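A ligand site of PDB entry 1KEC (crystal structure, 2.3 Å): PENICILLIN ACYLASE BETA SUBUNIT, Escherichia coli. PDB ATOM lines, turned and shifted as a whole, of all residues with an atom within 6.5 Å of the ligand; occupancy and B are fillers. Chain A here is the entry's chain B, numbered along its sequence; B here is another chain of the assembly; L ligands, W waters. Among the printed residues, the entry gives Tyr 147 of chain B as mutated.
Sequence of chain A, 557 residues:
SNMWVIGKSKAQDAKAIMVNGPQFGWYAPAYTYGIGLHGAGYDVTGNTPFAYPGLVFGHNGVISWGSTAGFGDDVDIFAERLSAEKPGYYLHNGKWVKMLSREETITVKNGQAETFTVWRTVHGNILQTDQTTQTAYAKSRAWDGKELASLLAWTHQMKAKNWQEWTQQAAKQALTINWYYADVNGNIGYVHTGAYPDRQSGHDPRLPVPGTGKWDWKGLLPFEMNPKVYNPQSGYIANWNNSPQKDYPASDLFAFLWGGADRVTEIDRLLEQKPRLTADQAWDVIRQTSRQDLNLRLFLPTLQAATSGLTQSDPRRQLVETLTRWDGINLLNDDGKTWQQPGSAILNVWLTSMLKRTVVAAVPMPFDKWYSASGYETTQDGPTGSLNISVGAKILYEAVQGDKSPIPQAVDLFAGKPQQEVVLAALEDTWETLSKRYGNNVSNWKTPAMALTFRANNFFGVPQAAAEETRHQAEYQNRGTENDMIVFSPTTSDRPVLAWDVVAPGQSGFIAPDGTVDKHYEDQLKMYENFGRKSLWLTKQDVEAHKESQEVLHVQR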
ATOM      1  N   SER A   1     -14.188 -22.208 -28.271  1.00  0.00           N
ATOM      2  CA  SER A   1     -14.887 -22.255 -29.589  1.00  0.00           C
ATOM      3  C   SER A   1     -15.192 -20.877 -30.125  1.00  0.00           C
ATOM      4  O   SER A   1     -15.709 -20.020 -29.393  1.00  0.00           O
ATOM      5  CB  SER A   1     -16.205 -23.004 -29.464  1.00  0.00           C
ATOM      6  OG  SER A   1     -15.989 -24.294 -28.942  1.00  0.00           O
ATOM      7  N   ASN A   2     -14.902 -20.650 -31.407  1.00  0.00           N
ATOM      8  CA  ASN A   2     -15.245 -19.376 -32.004  1.00  0.00           C
ATOM      9  C   ASN A   2     -16.302 -19.495 -33.085  1.00  0.00           C
ATOM     10  O   ASN A   2     -16.640 -20.594 -33.548  1.00  0.00           O
ATOM     11  CB  ASN A   2     -14.028 -18.519 -32.414  1.00  0.00           C
ATOM     12  CG  ASN A   2     -12.981 -19.278 -33.246  1.00  0.00           C
ATOM     13  OD1 ASN A   2     -11.789 -19.015 -33.121  1.00  0.00           O
ATOM     14  ND2 ASN A   2     -13.426 -20.198 -34.085  1.00  0.00           N
ATOM     15  N   ASN A  20     -17.681 -21.366 -38.136  1.00  0.00           N
ATOM     16  CA  ASN A  20     -17.706 -21.957 -36.800  1.00  0.00           C
ATOM     17  C   ASN A  20     -16.432 -22.770 -36.571  1.00  0.00           C
ATOM     18  O   ASN A  20     -16.013 -23.500 -37.468  1.00  0.00           O
ATOM     19  CB  ASN A  20     -18.881 -22.942 -36.727  1.00  0.00           C
ATOM     20  CG  ASN A  20     -19.477 -23.098 -35.308  1.00  0.00           C
ATOM     21  OD1 ASN A  20     -20.587 -23.604 -35.177  1.00  0.00           O
ATOM     22  ND2 ASN A  20     -18.749 -22.674 -34.252  1.00  0.00           N
ATOM     23  N   PRO A  22     -15.560 -24.961 -33.412  1.00  0.00           N
ATOM     24  CA  PRO A  22     -15.809 -25.509 -32.076  1.00  0.00           C
ATOM     25  C   PRO A  22     -14.518 -26.122 -31.518  1.00  0.00           C
ATOM     26  O   PRO A  22     -13.900 -26.928 -32.226  1.00  0.00           O
ATOM     27  CB  PRO A  22     -16.843 -26.604 -32.356  1.00  0.00           C
ATOM     28  CG  PRO A  22     -16.483 -27.044 -33.759  1.00  0.00           C
ATOM     29  CD  PRO A  22     -16.227 -25.739 -34.462  1.00  0.00           C
ATOM     30  N   GLN A  23     -14.118 -25.761 -30.295  1.00  0.00           N
ATOM     31  CA  GLN A  23     -12.841 -26.245 -29.759  1.00  0.00           C
ATOM     32  C   GLN A  23     -12.921 -27.362 -28.700  1.00  0.00           C
ATOM     33  O   GLN A  23     -12.797 -27.134 -27.486  1.00  0.00           O
ATOM     34  CB  GLN A  23     -11.961 -25.065 -29.305  1.00  0.00           C
ATOM     35  CG  GLN A  23     -11.511 -24.183 -30.497  1.00  0.00           C
ATOM     36  CD  GLN A  23     -10.731 -22.954 -30.028  1.00  0.00           C
ATOM     37  OE1 GLN A  23     -11.266 -22.133 -29.286  1.00  0.00           O
ATOM     38  NE2 GLN A  23      -9.451 -22.874 -30.398  1.00  0.00           N
ATOM     39  N   PHE A  24     -13.046 -28.576 -29.204  1.00  0.00           N
ATOM     40  CA  PHE A  24     -13.254 -29.750 -28.390  1.00  0.00           C
ATOM     41  C   PHE A  24     -11.966 -30.494 -27.971  1.00  0.00           C
ATOM     42  O   PHE A  24     -12.046 -31.530 -27.273  1.00  0.00           O
ATOM     43  CB  PHE A  24     -14.048 -30.746 -29.232  1.00  0.00           C
ATOM     44  CG  PHE A  24     -15.436 -30.310 -29.562  1.00  0.00           C
ATOM     45  CD1 PHE A  24     -16.402 -30.215 -28.580  1.00  0.00           C
ATOM     46  CD2 PHE A  24     -15.802 -30.086 -30.890  1.00  0.00           C
ATOM     47  CE1 PHE A  24     -17.714 -29.873 -28.896  1.00  0.00           C
ATOM     48  CE2 PHE A  24     -17.103 -29.748 -31.225  1.00  0.00           C
ATOM     49  CZ  PHE A  24     -18.066 -29.622 -30.223  1.00  0.00           C
ATOM     50  N   GLY A  25     -10.820 -30.014 -28.421  1.00  0.00           N
ATOM     51  CA  GLY A  25      -9.571 -30.748 -28.264  1.00  0.00           C
ATOM     52  C   GLY A  25      -9.350 -31.488 -29.589  1.00  0.00           C
ATOM     53  O   GLY A  25     -10.152 -31.344 -30.513  1.00  0.00           O
ATOM     54  N   PRO A  49     -20.599 -33.898 -33.254  1.00  0.00           N
ATOM     55  CA  PRO A  49     -19.801 -34.686 -32.294  1.00  0.00           C
ATOM     56  C   PRO A  49     -20.405 -36.053 -31.974  1.00  0.00           C
ATOM     57  O   PRO A  49     -21.608 -36.124 -31.761  1.00  0.00           O
ATOM     58  CB  PRO A  49     -19.811 -33.815 -31.032  1.00  0.00           C
ATOM     59  CG  PRO A  49     -20.140 -32.459 -31.529  1.00  0.00           C
ATOM     60  CD  PRO A  49     -21.109 -32.654 -32.666  1.00  0.00           C
ATOM     61  N   VAL A  56     -24.855 -30.637 -34.987  1.00  0.00           N
ATOM     62  CA  VAL A  56     -24.534 -29.353 -34.366  1.00  0.00           C
ATOM     63  C   VAL A  56     -23.990 -28.329 -35.355  1.00  0.00           C
ATOM     64  O   VAL A  56     -24.078 -27.143 -35.120  1.00  0.00           O
ATOM     65  CB  VAL A  56     -23.526 -29.511 -33.213  1.00  0.00           C
ATOM     66  CG1 VAL A  56     -23.196 -28.164 -32.603  1.00  0.00           C
ATOM     67  CG2 VAL A  56     -24.068 -30.458 -32.165  1.00  0.00           C
ATOM     68  N   PHE A  57     -23.396 -28.787 -36.448  1.00  0.00           N
ATOM     69  CA  PHE A  57     -22.820 -27.879 -37.425  1.00  0.00           C
ATOM     70  C   PHE A  57     -23.312 -28.282 -38.812  1.00  0.00           C
ATOM     71  O   PHE A  57     -22.919 -29.326 -39.326  1.00  0.00           O
ATOM     72  CB  PHE A  57     -21.292 -27.935 -37.354  1.00  0.00           C
ATOM     73  CG  PHE A  57     -20.756 -27.921 -35.951  1.00  0.00           C
ATOM     74  CD1 PHE A  57     -20.689 -26.736 -35.240  1.00  0.00           C
ATOM     75  CD2 PHE A  57     -20.317 -29.087 -35.342  1.00  0.00           C
ATOM     76  CE1 PHE A  57     -20.203 -26.696 -33.960  1.00  0.00           C
ATOM     77  CE2 PHE A  57     -19.823 -29.073 -34.042  1.00  0.00           C
ATOM     78  CZ  PHE A  57     -19.768 -27.871 -33.351  1.00  0.00           C
ATOM     79  N   SER A  67     -22.743 -23.664 -32.940  1.00  0.00           N
ATOM     80  CA  SER A  67     -22.739 -23.546 -31.499  1.00  0.00           C
ATOM     81  C   SER A  67     -21.362 -23.233 -30.967  1.00  0.00           C
ATOM     82  O   SER A  67     -20.352 -23.463 -31.656  1.00  0.00           O
ATOM     83  CB  SER A  67     -23.181 -24.872 -30.853  1.00  0.00           C
ATOM     84  OG  SER A  67     -24.587 -25.065 -30.907  1.00  0.00           O
ATOM     85  N   THR A  68     -21.358 -22.702 -29.741  1.00  0.00           N
ATOM     86  CA  THR A  68     -20.194 -22.521 -28.886  1.00  0.00           C
ATOM     87  C   THR A  68     -20.771 -22.664 -27.497  1.00  0.00           C
ATOM     88  O   THR A  68     -21.947 -22.337 -27.276  1.00  0.00           O
ATOM     89  CB  THR A  68     -19.489 -21.138 -29.052  1.00  0.00           C
ATOM     90  OG1 THR A  68     -20.352 -20.065 -28.656  1.00  0.00           O
ATOM     91  CG2 THR A  68     -19.187 -20.860 -30.524  1.00  0.00           C
ATOM     92  N   ALA A  69     -19.993 -23.197 -26.560  1.00  0.00           N
ATOM     93  CA  ALA A  69     -20.484 -23.372 -25.196  1.00  0.00           C
ATOM     94  C   ALA A  69     -20.819 -22.000 -24.643  1.00  0.00           C
ATOM     95  O   ALA A  69     -20.082 -21.056 -24.833  1.00  0.00           O
ATOM     96  CB  ALA A  69     -19.432 -24.060 -24.337  1.00  0.00           C
ATOM     97  N   GLY A  70     -21.957 -21.897 -23.958  1.00  0.00           N
ATOM     98  CA  GLY A  70     -22.399 -20.652 -23.377  1.00  0.00           C
ATOM     99  C   GLY A  70     -21.748 -20.247 -22.065  1.00  0.00           C
ATOM    100  O   GLY A  70     -21.528 -19.067 -21.807  1.00  0.00           O
ATOM    101  N   PHE A  71     -21.445 -21.238 -21.222  1.00  0.00           N
ATOM    102  CA  PHE A  71     -20.846 -20.964 -19.920  1.00  0.00           C
ATOM    103  C   PHE A  71     -21.664 -20.006 -19.051  1.00  0.00           C
ATOM    104  O   PHE A  71     -21.094 -19.144 -18.386  1.00  0.00           O
ATOM    105  CB  PHE A  71     -19.431 -20.407 -20.069  1.00  0.00           C
ATOM    106  CG  PHE A  71     -18.413 -21.456 -20.429  1.00  0.00           C
ATOM    107  CD1 PHE A  71     -17.809 -22.205 -19.437  1.00  0.00           C
ATOM    108  CD2 PHE A  71     -18.094 -21.722 -21.745  1.00  0.00           C
ATOM    109  CE1 PHE A  71     -16.874 -23.193 -19.750  1.00  0.00           C
ATOM    110  CE2 PHE A  71     -17.172 -22.692 -22.079  1.00  0.00           C
ATOM    111  CZ  PHE A  71     -16.565 -23.431 -21.067  1.00  0.00           C
ATOM    112  N   TRP A 154     -32.024 -30.153 -30.492  1.00  0.00           N
ATOM    113  CA  TRP A 154     -30.909 -30.054 -31.429  1.00  0.00           C
ATOM    114  C   TRP A 154     -31.190 -30.794 -32.754  1.00  0.00           C
ATOM    115  O   TRP A 154     -30.592 -30.486 -33.795  1.00  0.00           O
ATOM    116  CB  TRP A 154     -29.640 -30.612 -30.793  1.00  0.00           C
ATOM    117  CG  TRP A 154     -28.467 -29.671 -30.816  1.00  0.00           C
ATOM    118  CD1 TRP A 154     -28.007 -28.940 -31.876  1.00  0.00           C
ATOM    119  CD2 TRP A 154     -27.582 -29.379 -29.723  1.00  0.00           C
ATOM    120  NE1 TRP A 154     -26.909 -28.210 -31.509  1.00  0.00           N
ATOM    121  CE2 TRP A 154     -26.624 -28.462 -30.184  1.00  0.00           C
ATOM    122  CE3 TRP A 154     -27.528 -29.785 -28.385  1.00  0.00           C
ATOM    123  CZ2 TRP A 154     -25.604 -27.966 -29.368  1.00  0.00           C
ATOM    124  CZ3 TRP A 154     -26.504 -29.302 -27.569  1.00  0.00           C
ATOM    125  CH2 TRP A 154     -25.562 -28.399 -28.071  1.00  0.00           C
ATOM    126  N   THR A 176     -26.470 -25.128 -21.323  1.00  0.00           N
ATOM    127  CA  THR A 176     -26.027 -23.762 -21.549  1.00  0.00           C
ATOM    128  C   THR A 176     -25.159 -23.650 -22.807  1.00  0.00           C
ATOM    129  O   THR A 176     -23.934 -23.737 -22.748  1.00  0.00           O
ATOM    130  CB  THR A 176     -25.317 -23.174 -20.296  1.00  0.00           C
ATOM    131  OG1 THR A 176     -24.884 -21.836 -20.572  1.00  0.00           O
ATOM    132  CG2 THR A 176     -24.023 -23.920 -19.987  1.00  0.00           C
ATOM    133  N   ILE A 177     -25.822 -23.494 -23.956  1.00  0.00           N
ATOM    134  CA  ILE A 177     -25.133 -23.406 -25.220  1.00  0.00           C
ATOM    135  C   ILE A 177     -25.511 -22.157 -26.038  1.00  0.00           C
ATOM    136  O   ILE A 177     -26.684 -21.784 -26.119  1.00  0.00           O
ATOM    137  CB  ILE A 177     -25.432 -24.665 -26.051  1.00  0.00           C
ATOM    138  CG1 ILE A 177     -25.482 -25.918 -25.160  1.00  0.00           C
ATOM    139  CG2 ILE A 177     -24.423 -24.846 -27.180  1.00  0.00           C
ATOM    140  CD1 ILE A 177     -24.133 -26.447 -24.730  1.00  0.00           C
ATOM    141  N   ASN A 178     -24.517 -21.501 -26.646  1.00  0.00           N
ATOM    142  CA  ASN A 178     -24.809 -20.426 -27.579  1.00  0.00           C
ATOM    143  C   ASN A 178     -25.202 -21.056 -28.909  1.00  0.00           C
ATOM    144  O   ASN A 178     -24.435 -21.860 -29.441  1.00  0.00           O
ATOM    145  CB  ASN A 178     -23.550 -19.581 -27.817  1.00  0.00           C
ATOM    146  CG  ASN A 178     -23.123 -18.799 -26.587  1.00  0.00           C
ATOM    147  OD1 ASN A 178     -23.944 -18.138 -25.916  1.00  0.00           O
ATOM    148  ND2 ASN A 178     -21.832 -18.842 -26.285  1.00  0.00           N
ATOM    149  N   ASN A 241     -16.674 -17.795 -26.591  1.00  0.00           N
ATOM    150  CA  ASN A 241     -17.034 -18.133 -25.211  1.00  0.00           C
ATOM    151  C   ASN A 241     -17.046 -16.890 -24.303  1.00  0.00           C
ATOM    152  O   ASN A 241     -16.933 -17.001 -23.076  1.00  0.00           O
ATOM    153  CB  ASN A 241     -16.112 -19.201 -24.613  1.00  0.00           C
ATOM    154  CG  ASN A 241     -16.033 -20.466 -25.489  1.00  0.00           C
ATOM    155  OD1 ASN A 241     -14.958 -20.797 -25.993  1.00  0.00           O
ATOM    156  ND2 ASN A 241     -17.162 -21.171 -25.637  1.00  0.00           N
ATOM    157  N   ARG A 263     -10.601 -12.636 -25.360  1.00  0.00           N
ATOM    158  CA  ARG A 263     -10.080 -12.989 -26.677  1.00  0.00           C
ATOM    159  C   ARG A 263     -11.031 -12.670 -27.809  1.00  0.00           C
ATOM    160  O   ARG A 263     -10.598 -12.592 -28.953  1.00  0.00           O
ATOM    161  CB  ARG A 263      -9.722 -14.476 -26.748  1.00  0.00           C
ATOM    162  CG  ARG A 263     -10.896 -15.451 -26.595  1.00  0.00           C
ATOM    163  CD  ARG A 263     -10.407 -16.871 -26.382  1.00  0.00           C
ATOM    164  NE  ARG A 263     -11.474 -17.855 -26.204  1.00  0.00           N
ATOM    165  CZ  ARG A 263     -11.252 -19.124 -25.863  1.00  0.00           C
ATOM    166  NH1 ARG A 263      -9.989 -19.530 -25.668  1.00  0.00           N
ATOM    167  NH2 ARG A 263     -12.269 -19.986 -25.724  1.00  0.00           N
ATOM    168  N   MET B 143     -21.755 -34.213 -23.989  1.00  0.00           N
ATOM    169  CA  MET B 143     -22.135 -32.823 -24.238  1.00  0.00           C
ATOM    170  C   MET B 143     -22.590 -32.157 -22.952  1.00  0.00           C
ATOM    171  O   MET B 143     -21.978 -31.203 -22.496  1.00  0.00           O
ATOM    172  CB  MET B 143     -23.206 -32.724 -25.353  1.00  0.00           C
ATOM    173  CG  MET B 143     -23.764 -31.314 -25.629  1.00  0.00           C
ATOM    174  SD  MET B 143     -22.552 -30.065 -26.143  1.00  0.00           S
ATOM    175  CE  MET B 143     -22.262 -30.490 -27.809  1.00  0.00           C
ATOM    176  N   ARG B 146     -19.860 -32.693 -20.116  1.00  0.00           N
ATOM    177  CA  ARG B 146     -18.563 -32.088 -20.351  1.00  0.00           C
ATOM    178  C   ARG B 146     -18.665 -30.569 -20.410  1.00  0.00           C
ATOM    179  O   ARG B 146     -17.788 -29.867 -19.901  1.00  0.00           O
ATOM    180  CB  ARG B 146     -17.973 -32.619 -21.663  1.00  0.00           C
ATOM    181  CG  ARG B 146     -16.552 -32.131 -21.952  1.00  0.00           C
ATOM    182  CD  ARG B 146     -15.933 -32.666 -23.223  1.00  0.00           C
ATOM    183  NE  ARG B 146     -14.550 -32.215 -23.333  1.00  0.00           N
ATOM    184  CZ  ARG B 146     -13.812 -32.287 -24.424  1.00  0.00           C
ATOM    185  NH1 ARG B 146     -14.295 -32.830 -25.548  1.00  0.00           N
ATOM    186  NH2 ARG B 146     -12.569 -31.814 -24.399  1.00  0.00           N
ATOM    187  N   TYR B 147     -19.742 -30.071 -21.018  1.00  0.00           N
ATOM    188  CA  TYR B 147     -19.854 -28.635 -21.266  1.00  0.00           C
ATOM    189  C   TYR B 147     -20.965 -27.877 -20.507  1.00  0.00           C
ATOM    190  O   TYR B 147     -20.969 -26.651 -20.499  1.00  0.00           O
ATOM    191  CB  TYR B 147     -19.935 -28.391 -22.773  1.00  0.00           C
ATOM    192  CG  TYR B 147     -18.658 -28.785 -23.499  1.00  0.00           C
ATOM    193  CD1 TYR B 147     -18.684 -29.664 -24.563  1.00  0.00           C
ATOM    194  CD2 TYR B 147     -17.417 -28.282 -23.095  1.00  0.00           C
ATOM    195  CE1 TYR B 147     -17.531 -30.031 -25.204  1.00  0.00           C
ATOM    196  CE2 TYR B 147     -16.257 -28.653 -23.716  1.00  0.00           C
ATOM    197  CZ  TYR B 147     -16.318 -29.536 -24.780  1.00  0.00           C
ATOM    198  OH  TYR B 147     -15.186 -29.904 -25.452  1.00  0.00           O
HETATM  199  O1  LIG L   1     -17.309 -24.015 -26.775  1.00  0.00           O
HETATM  200  C1  LIG L   1     -17.011 -25.069 -26.003  1.00  0.00           C
HETATM  201  O2  LIG L   1     -16.392 -24.914 -24.959  1.00  0.00           O
HETATM  202  C2  LIG L   1     -17.384 -26.463 -26.404  1.00  0.00           C
HETATM  203  C3  LIG L   1     -16.181 -27.077 -27.131  1.00  0.00           C
HETATM  204  C4  LIG L   1     -18.646 -26.564 -27.194  1.00  0.00           C
HETATM  205  C5  LIG L   1     -19.788 -27.091 -26.583  1.00  0.00           C
HETATM  206  C6  LIG L   1     -20.990 -27.222 -27.280  1.00  0.00           C
HETATM  207  C7  LIG L   1     -21.057 -26.842 -28.618  1.00  0.00           C
HETATM  208  C8  LIG L   1     -19.914 -26.315 -29.248  1.00  0.00           C
HETATM  209  C9  LIG L   1     -18.713 -26.184 -28.531  1.00  0.00           C
HETATM  210  O   HOH W   1     -14.077 -24.207 -26.175  1.00  0.00           O
HETATM  211  O   HOH W   2     -14.363 -25.811 -23.068  1.00  0.00           O
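N of Ser 1 sits at hydrogen-bond distance from OD1 of Asn 241 (2.8 Å).
OG of Ser 1 is in hydrogen-bond range of N of Gln 23 (2.7 Å).
O of Ala 69 is in hydrogen-bond range of ND2 of Asn 241, at 3.0 Å.
The backbone carbonyl oxygen of Ala 69 sits at hydrogen-bond distance from the side-chain amide nitrogen of Asn 178.
OD1 of Asn 241 lies within hydrogen-bond range of NH2 of Arg 263 (2.8 Å).
The side-chain hydroxyl (OH) of Tyr 147 of chain B lies close to the guanidinium group (NH1) of Arg 146 of chain B, at 3.1 Å.
O of Phe 24 lies within hydrogen-bond range of NH2 of Arg 146 of chain B.
The backbone NH (N) of Ser 67 lies within hydrogen-bond range of the side-chain amide oxygen (OD1) of Asn 20 (3.1 Å).
Water W1 lies within hydrogen-bond range of an oxygen (O2) of the ligand (2.7 Å), the backbone NH of Ser 1 (2.9 Å) and the backbone carbonyl oxygen of Gln 23 (3.5 Å).
O1 of the ligand sits at hydrogen-bond distance from OG of Ser 1 (2.6 Å).
An oxygen (O1) of the ligand sits at hydrogen-bond distance from the backbone NH (N) of Ala 69, at 2.8 Å.
ND2 of Asn 241 lies within hydrogen-bond range of O1 of the ligand, at 3.1 Å.
Gln 23 touches the ligand.
CD1 of Phe 24 touches C3 of the ligand, 3.5 Å away.
Ser 67 touches the ligand (CB to C7, 3.7 Å).
Thr 68 touches the ligand (C to O1, 3.8 Å).
CE2 of Phe 71 touches O2 of the ligand, at 3.7 Å.
Met 143 of chain B touches the ligand (SD to C6, 3.4 Å).
Tyr 147 of chain B touches the ligand (CZ to C3, 3.4 Å).
Hydrophobic or aromatic side chains that line the ligand: Phe 24, Ala 69, Phe 71, Met 143 of chain B and Tyr 147 of chain B.
Of the 24 residues printed, 10 come within 4 Å of the ligand.
The nearest printed residue that does not touch the ligand is Ile 177 (4.1 Å).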
